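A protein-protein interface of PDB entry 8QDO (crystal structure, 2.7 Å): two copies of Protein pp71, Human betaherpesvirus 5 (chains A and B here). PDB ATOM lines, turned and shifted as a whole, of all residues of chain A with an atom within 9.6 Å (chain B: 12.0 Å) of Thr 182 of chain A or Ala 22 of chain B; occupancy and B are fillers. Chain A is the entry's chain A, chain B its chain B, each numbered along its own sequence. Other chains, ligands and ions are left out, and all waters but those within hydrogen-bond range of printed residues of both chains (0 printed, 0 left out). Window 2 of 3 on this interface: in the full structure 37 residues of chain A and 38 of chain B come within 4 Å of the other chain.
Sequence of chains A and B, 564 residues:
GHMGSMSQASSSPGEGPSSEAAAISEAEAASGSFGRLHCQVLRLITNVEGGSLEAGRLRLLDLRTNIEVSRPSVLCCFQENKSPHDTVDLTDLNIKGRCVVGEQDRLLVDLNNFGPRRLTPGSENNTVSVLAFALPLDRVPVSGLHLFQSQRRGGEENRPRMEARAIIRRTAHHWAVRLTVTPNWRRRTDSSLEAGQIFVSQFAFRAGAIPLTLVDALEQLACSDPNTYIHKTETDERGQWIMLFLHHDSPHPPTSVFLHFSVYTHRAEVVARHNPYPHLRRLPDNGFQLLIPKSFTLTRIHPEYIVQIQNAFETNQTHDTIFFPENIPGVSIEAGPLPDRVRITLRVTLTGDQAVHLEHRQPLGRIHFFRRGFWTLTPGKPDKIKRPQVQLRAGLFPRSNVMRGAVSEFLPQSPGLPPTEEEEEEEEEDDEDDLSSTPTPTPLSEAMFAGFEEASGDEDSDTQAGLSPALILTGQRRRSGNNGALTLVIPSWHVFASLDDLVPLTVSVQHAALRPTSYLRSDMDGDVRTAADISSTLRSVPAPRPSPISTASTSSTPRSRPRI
The guanidinium group (NH2) of Arg 165 of chain A lies within salt-bridge range of the side-chain carboxylate (OE1) of Glu 26 of chain B (2.7 Å).
The side-chain hydroxyl of Thr 180 of chain A lies within hydrogen-bond range of the side-chain carboxylate of Glu 26 of chain B (2.9 Å).
The side-chain hydroxyl (OG1) of Thr 182 of chain A is in hydrogen-bond range of the side-chain carboxylate (OE2) of Glu 26 of chain B.
The side-chain hydroxyl (OG) of Ser 256 of chain A lies within hydrogen-bond range of the side-chain hydroxyl (OG) of Ser 25 of chain B (2.7 Å).
Of the printed residues of chain B, Arg 165 of chain A touches Glu 26.
Thr 180 of chain A touches two residues of chain B.
Of chain B, only Ala 22 (3.5 Å) and Glu 26 (3.2 Å) come within 4 Å of Thr 182 of chain A.
No residue of chain B comes within 4 Å of Pro 183 of chain A.
No residue of chain B comes within 4 Å of Asn 184 of chain A.
No residue of chain B comes within 4 Å of Thr 255 of chain A.
Ser 256 of chain A touches just these residues of chain B: Ser 25 and Glu 26.
No residue of chain B comes within 4 Å of Val 257 of chain A.
Printed residues of chain B within 4 Å of Phe 258 of chain A: Ala 29 and Ala 30.
No residue of chain A comes within 4 Å of Ser 19 of chain B.
No residue of chain A comes within 4 Å of Ala 21 of chain B.
No residue of chain A comes within 4 Å of Ala 23 of chain B.
Of the printed residues of chain A, Glu 26 of chain B touches Arg 165, Thr 180, Val 181, Thr 182 and Ser 256.
Of the printed residues of chain A, Ala 29 of chain B touches Phe 258 (3.7 Å).
Printed residues of chain A within 4 Å of Ala 30 of chain B: Thr 180 and Phe 258.
The nearest residue of chain B that does not touch Thr 182 of chain A is Ser 25 of chain B (4.1 Å).
The nearest residue of chain A that does not touch Ala 22 of chain B is Ser 256 of chain A (4.03 Å).
The nearest printed residue of chain A that does not touch Ala 29 of chain B is Ser 256 of chain A (4.1 Å).
Ala 30 of chain B touches Thr 180 of chain A.
Val 181 of chain A touches Glu 26 of chain B (C to OE2, 3.4 Å).
Thr 182 of chain A touches Ala 22 of chain B.
Glu 26 of chain B touches Ser 256 of chain A (CG to OG, 3.6 Å).
O of Ala 29 of chain B touches CB of Phe 258 of chain A (3.7 Å).
CB of Phe 258 of chain A touches CA of Ala 30 of chain B, 3.8 Å away.
No position is printed for both chains.
Of the 10 pairs that touch across the chains among the printed residues, none has its exchanged pair printed and touching as well.
Of the 14 printed residues of chain B, 5 touch a printed residue of chain A.
Hydrophobic or aromatic side chains of chain B within 4 Å of the printed part of chain A: Ala 22, Ala 29 and Ala 30.
Of the 24 printed residues of chain A, 6 touch a printed residue of chain B.
Hydrophobic or aromatic side chains of chain A within 4 Å of the printed part of chain B: Phe 258.
The backbone carbonyl oxygen (O) of Arg 165 of chain A sits at hydrogen-bond distance from the backbone NH (N) of Thr 180 of chain A.
The backbone NH (N) of Val 257 of chain A sits at hydrogen-bond distance from the backbone carbonyl oxygen (O) of Val 181 of chain A, 3.0 Å away.
The side-chain hydroxyl (OG1) of Thr 182 of chain A sits at hydrogen-bond distance from the side-chain hydroxyl (OG) of Ser 256 of chain A (2.7 Å).
The backbone carbonyl oxygen (O) of Ala 21 of chain B is in hydrogen-bond range of the side-chain hydroxyl (OG) of Ser 25 of chain B (3.2 Å).
The side-chain hydroxyl (OG) of Ser 25 of chain B lies within hydrogen-bond range of the backbone carbonyl oxygen (O) of Ala 22 of chain B (3.0 Å).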
ATOM      1  N   ARG A 161     -12.413 -10.723  22.593  1.00  0.00           N
ATOM      2  CA  ARG A 161     -10.965 -10.627  22.391  1.00  0.00           C
ATOM      3  C   ARG A 161     -10.141 -11.687  23.127  1.00  0.00           C
ATOM      4  O   ARG A 161      -9.487 -11.401  24.141  1.00  0.00           O
ATOM      5  CB  ARG A 161     -10.498  -9.206  22.743  1.00  0.00           C
ATOM      6  CG  ARG A 161     -10.601  -8.828  24.200  1.00  0.00           C
ATOM      7  CD  ARG A 161     -10.284  -7.365  24.403  1.00  0.00           C
ATOM      8  NE  ARG A 161     -10.546  -6.955  25.777  1.00  0.00           N
ATOM      9  CZ  ARG A 161      -9.752  -7.208  26.809  1.00  0.00           C
ATOM     10  NH1 ARG A 161      -8.636  -7.911  26.669  1.00  0.00           N
ATOM     11  NH2 ARG A 161     -10.093  -6.757  28.014  1.00  0.00           N
ATOM     12  N   MET A 162     -10.147 -12.914  22.589  1.00  0.00           N
ATOM     13  CA  MET A 162      -9.420 -14.052  23.152  1.00  0.00           C
ATOM     14  C   MET A 162      -7.920 -13.846  22.991  1.00  0.00           C
ATOM     15  O   MET A 162      -7.263 -14.510  22.182  1.00  0.00           O
ATOM     16  CB  MET A 162      -9.871 -15.367  22.509  1.00  0.00           C
ATOM     17  CG  MET A 162     -11.303 -15.755  22.876  1.00  0.00           C
ATOM     18  SD  MET A 162     -11.669 -15.458  24.631  1.00  0.00           S
ATOM     19  CE  MET A 162     -13.450 -15.230  24.580  1.00  0.00           C
ATOM     20  N   GLU A 163      -7.377 -12.932  23.791  1.00  0.00           N
ATOM     21  CA  GLU A 163      -6.025 -12.442  23.570  1.00  0.00           C
ATOM     22  C   GLU A 163      -4.976 -13.504  23.884  1.00  0.00           C
ATOM     23  O   GLU A 163      -3.985 -13.633  23.155  1.00  0.00           O
ATOM     24  CB  GLU A 163      -5.808 -11.193  24.422  1.00  0.00           C
ATOM     25  CG  GLU A 163      -4.389 -10.667  24.433  1.00  0.00           C
ATOM     26  CD  GLU A 163      -4.309  -9.316  25.096  1.00  0.00           C
ATOM     27  OE1 GLU A 163      -5.388  -8.775  25.435  1.00  0.00           O
ATOM     28  OE2 GLU A 163      -3.181  -8.809  25.293  1.00  0.00           O
ATOM     29  N   ALA A 164      -5.170 -14.275  24.951  1.00  0.00           N
ATOM     30  CA  ALA A 164      -4.168 -15.225  25.420  1.00  0.00           C
ATOM     31  C   ALA A 164      -4.463 -16.633  24.917  1.00  0.00           C
ATOM     32  O   ALA A 164      -5.626 -17.030  24.796  1.00  0.00           O
ATOM     33  CB  ALA A 164      -4.095 -15.226  26.949  1.00  0.00           C
ATOM     34  N   ARG A 165      -3.401 -17.382  24.628  1.00  0.00           N
ATOM     35  CA  ARG A 165      -3.504 -18.766  24.179  1.00  0.00           C
ATOM     36  C   ARG A 165      -3.147 -19.688  25.340  1.00  0.00           C
ATOM     37  O   ARG A 165      -2.056 -19.581  25.915  1.00  0.00           O
ATOM     38  CB  ARG A 165      -2.592 -19.019  22.980  1.00  0.00           C
ATOM     39  CG  ARG A 165      -2.861 -18.076  21.818  1.00  0.00           C
ATOM     40  CD  ARG A 165      -2.005 -18.403  20.606  1.00  0.00           C
ATOM     41  NE  ARG A 165      -0.585 -18.459  20.940  1.00  0.00           N
ATOM     42  CZ  ARG A 165       0.203 -17.400  21.080  1.00  0.00           C
ATOM     43  NH1 ARG A 165      -0.263 -16.167  20.944  1.00  0.00           N
ATOM     44  NH2 ARG A 165       1.490 -17.583  21.361  1.00  0.00           N
ATOM     45  N   LEU A 179      -0.373 -20.871  30.067  1.00  0.00           N
ATOM     46  CA  LEU A 179      -0.870 -19.739  29.306  1.00  0.00           C
ATOM     47  C   LEU A 179       0.257 -18.753  29.041  1.00  0.00           C
ATOM     48  O   LEU A 179       1.055 -18.463  29.933  1.00  0.00           O
ATOM     49  CB  LEU A 179      -2.022 -19.080  30.082  1.00  0.00           C
ATOM     50  CG  LEU A 179      -2.596 -17.724  29.709  1.00  0.00           C
ATOM     51  CD1 LEU A 179      -4.016 -17.608  30.234  1.00  0.00           C
ATOM     52  CD2 LEU A 179      -1.720 -16.647  30.300  1.00  0.00           C
ATOM     53  N   THR A 180       0.337 -18.263  27.807  1.00  0.00           N
ATOM     54  CA  THR A 180       1.231 -17.163  27.477  1.00  0.00           C
ATOM     55  C   THR A 180       0.429 -16.017  26.885  1.00  0.00           C
ATOM     56  O   THR A 180      -0.611 -16.226  26.247  1.00  0.00           O
ATOM     57  CB  THR A 180       2.330 -17.576  26.503  1.00  0.00           C
ATOM     58  OG1 THR A 180       1.735 -18.047  25.284  1.00  0.00           O
ATOM     59  CG2 THR A 180       3.203 -18.658  27.118  1.00  0.00           C
ATOM     60  N   VAL A 181       0.927 -14.801  27.096  1.00  0.00           N
ATOM     61  CA  VAL A 181       0.210 -13.604  26.684  1.00  0.00           C
ATOM     62  C   VAL A 181       1.203 -12.460  26.594  1.00  0.00           C
ATOM     63  O   VAL A 181       2.221 -12.444  27.294  1.00  0.00           O
ATOM     64  CB  VAL A 181      -0.942 -13.285  27.668  1.00  0.00           C
ATOM     65  CG1 VAL A 181      -0.375 -12.959  29.043  1.00  0.00           C
ATOM     66  CG2 VAL A 181      -1.785 -12.144  27.146  1.00  0.00           C
ATOM     67  N   THR A 182       0.915 -11.508  25.702  1.00  0.00           N
ATOM     68  CA  THR A 182       1.610 -10.225  25.639  1.00  0.00           C
ATOM     69  C   THR A 182       0.631  -9.141  26.069  1.00  0.00           C
ATOM     70  O   THR A 182      -0.098  -8.586  25.235  1.00  0.00           O
ATOM     71  CB  THR A 182       2.157  -9.942  24.239  1.00  0.00           C
ATOM     72  OG1 THR A 182       3.096 -10.962  23.871  1.00  0.00           O
ATOM     73  CG2 THR A 182       2.847  -8.594  24.219  1.00  0.00           C
ATOM     74  N   PRO A 183       0.565  -8.812  27.355  1.00  0.00           N
ATOM     75  CA  PRO A 183      -0.507  -7.947  27.852  1.00  0.00           C
ATOM     76  C   PRO A 183      -0.267  -6.479  27.532  1.00  0.00           C
ATOM     77  O   PRO A 183       0.838  -6.056  27.187  1.00  0.00           O
ATOM     78  CB  PRO A 183      -0.469  -8.184  29.366  1.00  0.00           C
ATOM     79  CG  PRO A 183       0.958  -8.532  29.643  1.00  0.00           C
ATOM     80  CD  PRO A 183       1.462  -9.268  28.434  1.00  0.00           C
ATOM     81  N   ASN A 184      -1.342  -5.701  27.664  1.00  0.00           N
ATOM     82  CA  ASN A 184      -1.299  -4.248  27.517  1.00  0.00           C
ATOM     83  C   ASN A 184      -1.280  -3.638  28.916  1.00  0.00           C
ATOM     84  O   ASN A 184      -2.327  -3.460  29.545  1.00  0.00           O
ATOM     85  CB  ASN A 184      -2.486  -3.738  26.705  1.00  0.00           C
ATOM     86  CG  ASN A 184      -2.486  -4.260  25.277  1.00  0.00           C
ATOM     87  OD1 ASN A 184      -1.433  -4.583  24.715  1.00  0.00           O
ATOM     88  ND2 ASN A 184      -3.671  -4.344  24.680  1.00  0.00           N
ATOM     89  N   TRP A 185      -0.085  -3.328  29.405  1.00  0.00           N
ATOM     90  CA  TRP A 185       0.066  -2.812  30.755  1.00  0.00           C
ATOM     91  C   TRP A 185      -0.329  -1.344  30.816  1.00  0.00           C
ATOM     92  O   TRP A 185      -0.051  -0.575  29.895  1.00  0.00           O
ATOM     93  CB  TRP A 185       1.512  -2.964  31.231  1.00  0.00           C
ATOM     94  CG  TRP A 185       1.968  -4.376  31.428  1.00  0.00           C
ATOM     95  CD1 TRP A 185       2.847  -5.067  30.650  1.00  0.00           C
ATOM     96  CD2 TRP A 185       1.582  -5.265  32.484  1.00  0.00           C
ATOM     97  NE1 TRP A 185       3.029  -6.335  31.148  1.00  0.00           N
ATOM     98  CE2 TRP A 185       2.263  -6.482  32.274  1.00  0.00           C
ATOM     99  CE3 TRP A 185       0.724  -5.154  33.584  1.00  0.00           C
ATOM    100  CZ2 TRP A 185       2.111  -7.580  33.124  1.00  0.00           C
ATOM    101  CZ3 TRP A 185       0.577  -6.242  34.426  1.00  0.00           C
ATOM    102  CH2 TRP A 185       1.266  -7.438  34.191  1.00  0.00           C
ATOM    103  N   SER A 201      -2.986  -5.123  34.026  1.00  0.00           N
ATOM    104  CA  SER A 201      -3.404  -5.557  32.700  1.00  0.00           C
ATOM    105  C   SER A 201      -4.545  -6.549  32.872  1.00  0.00           C
ATOM    106  O   SER A 201      -4.911  -6.909  33.992  1.00  0.00           O
ATOM    107  CB  SER A 201      -2.241  -6.157  31.903  1.00  0.00           C
ATOM    108  OG  SER A 201      -1.747  -7.336  32.510  1.00  0.00           O
ATOM    109  N   GLN A 202      -5.134  -6.960  31.749  1.00  0.00           N
ATOM    110  CA  GLN A 202      -6.235  -7.916  31.779  1.00  0.00           C
ATOM    111  C   GLN A 202      -6.424  -8.517  30.392  1.00  0.00           C
ATOM    112  O   GLN A 202      -6.183  -7.854  29.380  1.00  0.00           O
ATOM    113  CB  GLN A 202      -7.538  -7.262  32.242  1.00  0.00           C
ATOM    114  CG  GLN A 202      -8.173  -6.373  31.191  1.00  0.00           C
ATOM    115  CD  GLN A 202      -9.421  -5.668  31.686  1.00  0.00           C
ATOM    116  OE1 GLN A 202      -9.345  -4.656  32.387  1.00  0.00           O
ATOM    117  NE2 GLN A 202     -10.583  -6.214  31.334  1.00  0.00           N
ATOM    118  N   PHE A 203      -6.875  -9.771  30.361  1.00  0.00           N
ATOM    119  CA  PHE A 203      -7.079 -10.516  29.121  1.00  0.00           C
ATOM    120  C   PHE A 203      -7.963 -11.717  29.428  1.00  0.00           C
ATOM    121  O   PHE A 203      -8.311 -11.969  30.583  1.00  0.00           O
ATOM    122  CB  PHE A 203      -5.750 -10.948  28.502  1.00  0.00           C
ATOM    123  CG  PHE A 203      -4.846 -11.670  29.454  1.00  0.00           C
ATOM    124  CD1 PHE A 203      -4.916 -13.046  29.586  1.00  0.00           C
ATOM    125  CD2 PHE A 203      -3.923 -10.974  30.219  1.00  0.00           C
ATOM    126  CE1 PHE A 203      -4.081 -13.717  30.469  1.00  0.00           C
ATOM    127  CE2 PHE A 203      -3.088 -11.639  31.101  1.00  0.00           C
ATOM    128  CZ  PHE A 203      -3.170 -13.012  31.224  1.00  0.00           C
ATOM    129  N   ALA A 204      -8.337 -12.461  28.388  1.00  0.00           N
ATOM    130  CA  ALA A 204      -9.212 -13.612  28.562  1.00  0.00           C
ATOM    131  C   ALA A 204      -8.685 -14.787  27.754  1.00  0.00           C
ATOM    132  O   ALA A 204      -7.859 -14.627  26.853  1.00  0.00           O
ATOM    133  CB  ALA A 204     -10.661 -13.297  28.172  1.00  0.00           C
ATOM    134  N   LEU A 246      -4.122  -9.049  35.834  1.00  0.00           N
ATOM    135  CA  LEU A 246      -2.772  -9.164  36.370  1.00  0.00           C
ATOM    136  C   LEU A 246      -2.315  -7.856  37.007  1.00  0.00           C
ATOM    137  O   LEU A 246      -2.737  -6.766  36.615  1.00  0.00           O
ATOM    138  CB  LEU A 246      -1.774  -9.566  35.283  1.00  0.00           C
ATOM    139  CG  LEU A 246      -1.998 -10.884  34.542  1.00  0.00           C
ATOM    140  CD1 LEU A 246      -0.802 -11.224  33.653  1.00  0.00           C
ATOM    141  CD2 LEU A 246      -2.281 -12.004  35.521  1.00  0.00           C
ATOM    142  N   PRO A 253       7.177  -3.449  33.638  1.00  0.00           N
ATOM    143  CA  PRO A 253       6.398  -4.670  33.442  1.00  0.00           C
ATOM    144  C   PRO A 253       6.943  -5.471  32.277  1.00  0.00           C
ATOM    145  O   PRO A 253       7.460  -4.902  31.299  1.00  0.00           O
ATOM    146  CB  PRO A 253       4.981  -4.143  33.147  1.00  0.00           C
ATOM    147  CG  PRO A 253       5.195  -2.762  32.639  1.00  0.00           C
ATOM    148  CD  PRO A 253       6.380  -2.236  33.394  1.00  0.00           C
ATOM    149  N   PRO A 254       6.844  -6.796  32.327  1.00  0.00           N
ATOM    150  CA  PRO A 254       7.395  -7.619  31.247  1.00  0.00           C
ATOM    151  C   PRO A 254       6.518  -7.578  30.006  1.00  0.00           C
ATOM    152  O   PRO A 254       5.289  -7.491  30.079  1.00  0.00           O
ATOM    153  CB  PRO A 254       7.422  -9.024  31.861  1.00  0.00           C
ATOM    154  CG  PRO A 254       6.299  -9.005  32.851  1.00  0.00           C
ATOM    155  CD  PRO A 254       6.263  -7.611  33.410  1.00  0.00           C
ATOM    156  N   THR A 255       7.174  -7.661  28.848  1.00  0.00           N
ATOM    157  CA  THR A 255       6.441  -7.606  27.588  1.00  0.00           C
ATOM    158  C   THR A 255       5.552  -8.832  27.405  1.00  0.00           C
ATOM    159  O   THR A 255       4.397  -8.712  26.978  1.00  0.00           O
ATOM    160  CB  THR A 255       7.422  -7.447  26.428  1.00  0.00           C
ATOM    161  OG1 THR A 255       8.339  -8.545  26.426  1.00  0.00           O
ATOM    162  CG2 THR A 255       8.210  -6.154  26.588  1.00  0.00           C
ATOM    163  N   SER A 256       6.067 -10.022  27.721  1.00  0.00           N
ATOM    164  CA  SER A 256       5.277 -11.244  27.664  1.00  0.00           C
ATOM    165  C   SER A 256       5.408 -12.006  28.979  1.00  0.00           C
ATOM    166  O   SER A 256       6.430 -11.919  29.671  1.00  0.00           O
ATOM    167  CB  SER A 256       5.691 -12.123  26.477  1.00  0.00           C
ATOM    168  OG  SER A 256       5.313 -11.510  25.255  1.00  0.00           O
ATOM    169  N   VAL A 257       4.360 -12.763  29.312  1.00  0.00           N
ATOM    170  CA  VAL A 257       4.244 -13.444  30.597  1.00  0.00           C
ATOM    171  C   VAL A 257       3.791 -14.882  30.373  1.00  0.00           C
ATOM    172  O   VAL A 257       2.809 -15.120  29.662  1.00  0.00           O
ATOM    173  CB  VAL A 257       3.249 -12.713  31.521  1.00  0.00           C
ATOM    174  CG1 VAL A 257       3.018 -13.510  32.792  1.00  0.00           C
ATOM    175  CG2 VAL A 257       3.744 -11.311  31.837  1.00  0.00           C
ATOM    176  N   PHE A 258       4.491 -15.835  30.991  1.00  0.00           N
ATOM    177  CA  PHE A 258       4.016 -17.212  31.086  1.00  0.00           C
ATOM    178  C   PHE A 258       3.371 -17.441  32.451  1.00  0.00           C
ATOM    179  O   PHE A 258       3.898 -17.007  33.483  1.00  0.00           O
ATOM    180  CB  PHE A 258       5.152 -18.213  30.866  1.00  0.00           C
ATOM    181  CG  PHE A 258       4.814 -19.625  31.280  1.00  0.00           C
ATOM    182  CD1 PHE A 258       4.037 -20.433  30.465  1.00  0.00           C
ATOM    183  CD2 PHE A 258       5.287 -20.149  32.474  1.00  0.00           C
ATOM    184  CE1 PHE A 258       3.723 -21.728  30.839  1.00  0.00           C
ATOM    185  CE2 PHE A 258       4.980 -21.441  32.853  1.00  0.00           C
ATOM    186  CZ  PHE A 258       4.197 -22.232  32.036  1.00  0.00           C
ATOM    187  N   LEU A 259       2.217 -18.107  32.447  1.00  0.00           N
ATOM    188  CA  LEU A 259       1.479 -18.399  33.670  1.00  0.00           C
ATOM    189  C   LEU A 259       1.086 -19.866  33.712  1.00  0.00           C
ATOM    190  O   LEU A 259       0.574 -20.408  32.727  1.00  0.00           O
ATOM    191  CB  LEU A 259       0.217 -17.542  33.785  1.00  0.00           C
ATOM    192  CG  LEU A 259       0.323 -16.195  34.490  1.00  0.00           C
ATOM    193  CD1 LEU A 259      -1.007 -15.474  34.382  1.00  0.00           C
ATOM    194  CD2 LEU A 259       0.737 -16.364  35.939  1.00  0.00           C
ATOM    195  N   SER B  18      -0.465 -11.076  18.448  1.00  0.00           N
ATOM    196  CA  SER B  18      -0.257  -9.913  17.590  1.00  0.00           C
ATOM    197  C   SER B  18       0.740 -10.202  16.471  1.00  0.00           C
ATOM    198  O   SER B  18       0.480 -11.030  15.595  1.00  0.00           O
ATOM    199  CB  SER B  18       0.229  -8.719  18.416  1.00  0.00           C
ATOM    200  OG  SER B  18       0.542  -7.617  17.581  1.00  0.00           O
ATOM    201  N   SER B  19       1.886  -9.523  16.516  1.00  0.00           N
ATOM    202  CA  SER B  19       2.924  -9.735  15.521  1.00  0.00           C
ATOM    203  C   SER B  19       3.785 -10.934  15.907  1.00  0.00           C
ATOM    204  O   SER B  19       3.692 -11.473  17.014  1.00  0.00           O
ATOM    205  CB  SER B  19       3.791  -8.481  15.365  1.00  0.00           C
ATOM    206  OG  SER B  19       4.468  -8.152  16.569  1.00  0.00           O
ATOM    207  N   GLU B  20       4.643 -11.350  14.971  1.00  0.00           N
ATOM    208  CA  GLU B  20       5.535 -12.469  15.244  1.00  0.00           C
ATOM    209  C   GLU B  20       6.509 -12.144  16.369  1.00  0.00           C
ATOM    210  O   GLU B  20       7.059 -13.065  16.984  1.00  0.00           O
ATOM    211  CB  GLU B  20       6.288 -12.878  13.972  1.00  0.00           C
ATOM    212  CG  GLU B  20       6.380 -14.393  13.771  1.00  0.00           C
ATOM    213  CD  GLU B  20       7.575 -15.019  14.478  1.00  0.00           C
ATOM    214  OE1 GLU B  20       8.501 -14.271  14.863  1.00  0.00           O
ATOM    215  OE2 GLU B  20       7.588 -16.256  14.658  1.00  0.00           O
ATOM    216  N   ALA B  21       6.725 -10.858  16.658  1.00  0.00           N
ATOM    217  CA  ALA B  21       7.573 -10.494  17.787  1.00  0.00           C
ATOM    218  C   ALA B  21       6.929 -10.904  19.106  1.00  0.00           C
ATOM    219  O   ALA B  21       7.627 -11.317  20.040  1.00  0.00           O
ATOM    220  CB  ALA B  21       7.859  -8.994  17.764  1.00  0.00           C
ATOM    221  N   ALA B  22       5.600 -10.791  19.203  1.00  0.00           N
ATOM    222  CA  ALA B  22       4.895 -11.260  20.393  1.00  0.00           C
ATOM    223  C   ALA B  22       4.968 -12.776  20.530  1.00  0.00           C
ATOM    224  O   ALA B  22       5.022 -13.294  21.652  1.00  0.00           O
ATOM    225  CB  ALA B  22       3.437 -10.804  20.355  1.00  0.00           C
ATOM    226  N   ALA B  23       4.972 -13.502  19.410  1.00  0.00           N
ATOM    227  CA  ALA B  23       5.075 -14.958  19.468  1.00  0.00           C
ATOM    228  C   ALA B  23       6.439 -15.396  19.990  1.00  0.00           C
ATOM    229  O   ALA B  23       6.546 -16.411  20.690  1.00  0.00           O
ATOM    230  CB  ALA B  23       4.807 -15.561  18.090  1.00  0.00           C
ATOM    231  N   ILE B  24       7.497 -14.658  19.641  1.00  0.00           N
ATOM    232  CA  ILE B  24       8.844 -15.032  20.063  1.00  0.00           C
ATOM    233  C   ILE B  24       9.043 -14.757  21.551  1.00  0.00           C
ATOM    234  O   ILE B  24       9.641 -15.566  22.272  1.00  0.00           O
ATOM    235  CB  ILE B  24       9.892 -14.305  19.199  1.00  0.00           C
ATOM    236  CG1 ILE B  24       9.846 -14.829  17.759  1.00  0.00           C
ATOM    237  CG2 ILE B  24      11.290 -14.471  19.785  1.00  0.00           C
ATOM    238  CD1 ILE B  24      10.395 -16.236  17.591  1.00  0.00           C
ATOM    239  N   SER B  25       8.563 -13.609  22.036  1.00  0.00           N
ATOM    240  CA  SER B  25       8.729 -13.282  23.449  1.00  0.00           C
ATOM    241  C   SER B  25       7.915 -14.220  24.334  1.00  0.00           C
ATOM    242  O   SER B  25       8.357 -14.589  25.428  1.00  0.00           O
ATOM    243  CB  SER B  25       8.332 -11.830  23.695  1.00  0.00           C
ATOM    244  OG  SER B  25       7.039 -11.587  23.170  1.00  0.00           O
ATOM    245  N   GLU B  26       6.720 -14.607  23.883  1.00  0.00           N
ATOM    246  CA  GLU B  26       5.921 -15.557  24.649  1.00  0.00           C
ATOM    247  C   GLU B  26       6.621 -16.905  24.748  1.00  0.00           C
ATOM    248  O   GLU B  26       6.589 -17.553  25.800  1.00  0.00           O
ATOM    249  CB  GLU B  26       4.537 -15.711  24.018  1.00  0.00           C
ATOM    250  CG  GLU B  26       3.641 -14.489  24.198  1.00  0.00           C
ATOM    251  CD  GLU B  26       2.263 -14.687  23.602  1.00  0.00           C
ATOM    252  OE1 GLU B  26       1.895 -15.853  23.349  1.00  0.00           O
ATOM    253  OE2 GLU B  26       1.545 -13.683  23.388  1.00  0.00           O
ATOM    254  N   ALA B  27       7.261 -17.344  23.665  1.00  0.00           N
ATOM    255  CA  ALA B  27       7.987 -18.609  23.707  1.00  0.00           C
ATOM    256  C   ALA B  27       9.199 -18.522  24.629  1.00  0.00           C
ATOM    257  O   ALA B  27       9.509 -19.479  25.347  1.00  0.00           O
ATOM    258  CB  ALA B  27       8.410 -19.019  22.298  1.00  0.00           C
ATOM    259  N   GLU B  28       9.897 -17.384  24.632  1.00  0.00           N
ATOM    260  CA  GLU B  28      11.028 -17.239  25.543  1.00  0.00           C
ATOM    261  C   GLU B  28      10.567 -17.238  26.994  1.00  0.00           C
ATOM    262  O   GLU B  28      11.265 -17.758  27.873  1.00  0.00           O
ATOM    263  CB  GLU B  28      11.799 -15.960  25.230  1.00  0.00           C
ATOM    264  CG  GLU B  28      12.541 -16.005  23.912  1.00  0.00           C
ATOM    265  CD  GLU B  28      13.371 -14.764  23.674  1.00  0.00           C
ATOM    266  OE1 GLU B  28      13.515 -13.959  24.622  1.00  0.00           O
ATOM    267  OE2 GLU B  28      13.879 -14.597  22.544  1.00  0.00           O
ATOM    268  N   ALA B  29       9.393 -16.655  27.263  1.00  0.00           N
ATOM    269  CA  ALA B  29       8.846 -16.677  28.616  1.00  0.00           C
ATOM    270  C   ALA B  29       8.476 -18.092  29.041  1.00  0.00           C
ATOM    271  O   ALA B  29       8.748 -18.499  30.178  1.00  0.00           O
ATOM    272  CB  ALA B  29       7.630 -15.757  28.704  1.00  0.00           C
ATOM    273  N   ALA B  30       7.864 -18.860  28.138  1.00  0.00           N
ATOM    274  CA  ALA B  30       7.406 -20.192  28.514  1.00  0.00           C
ATOM    275  C   ALA B  30       8.578 -21.145  28.733  1.00  0.00           C
ATOM    276  O   ALA B  30       8.547 -21.967  29.656  1.00  0.00           O
ATOM    277  CB  ALA B  30       6.452 -20.735  27.451  1.00  0.00           C
ATOM    278  N   SER B  31       9.620 -21.056  27.903  1.00  0.00           N
ATOM    279  CA  SER B  31      10.721 -22.007  28.014  1.00  0.00           C
ATOM    280  C   SER B  31      11.756 -21.610  29.064  1.00  0.00           C
ATOM    281  O   SER B  31      12.515 -22.472  29.514  1.00  0.00           O
ATOM    282  CB  SER B  31      11.413 -22.186  26.661  1.00  0.00           C
ATOM    283  OG  SER B  31      12.136 -21.023  26.311  1.00  0.00           O
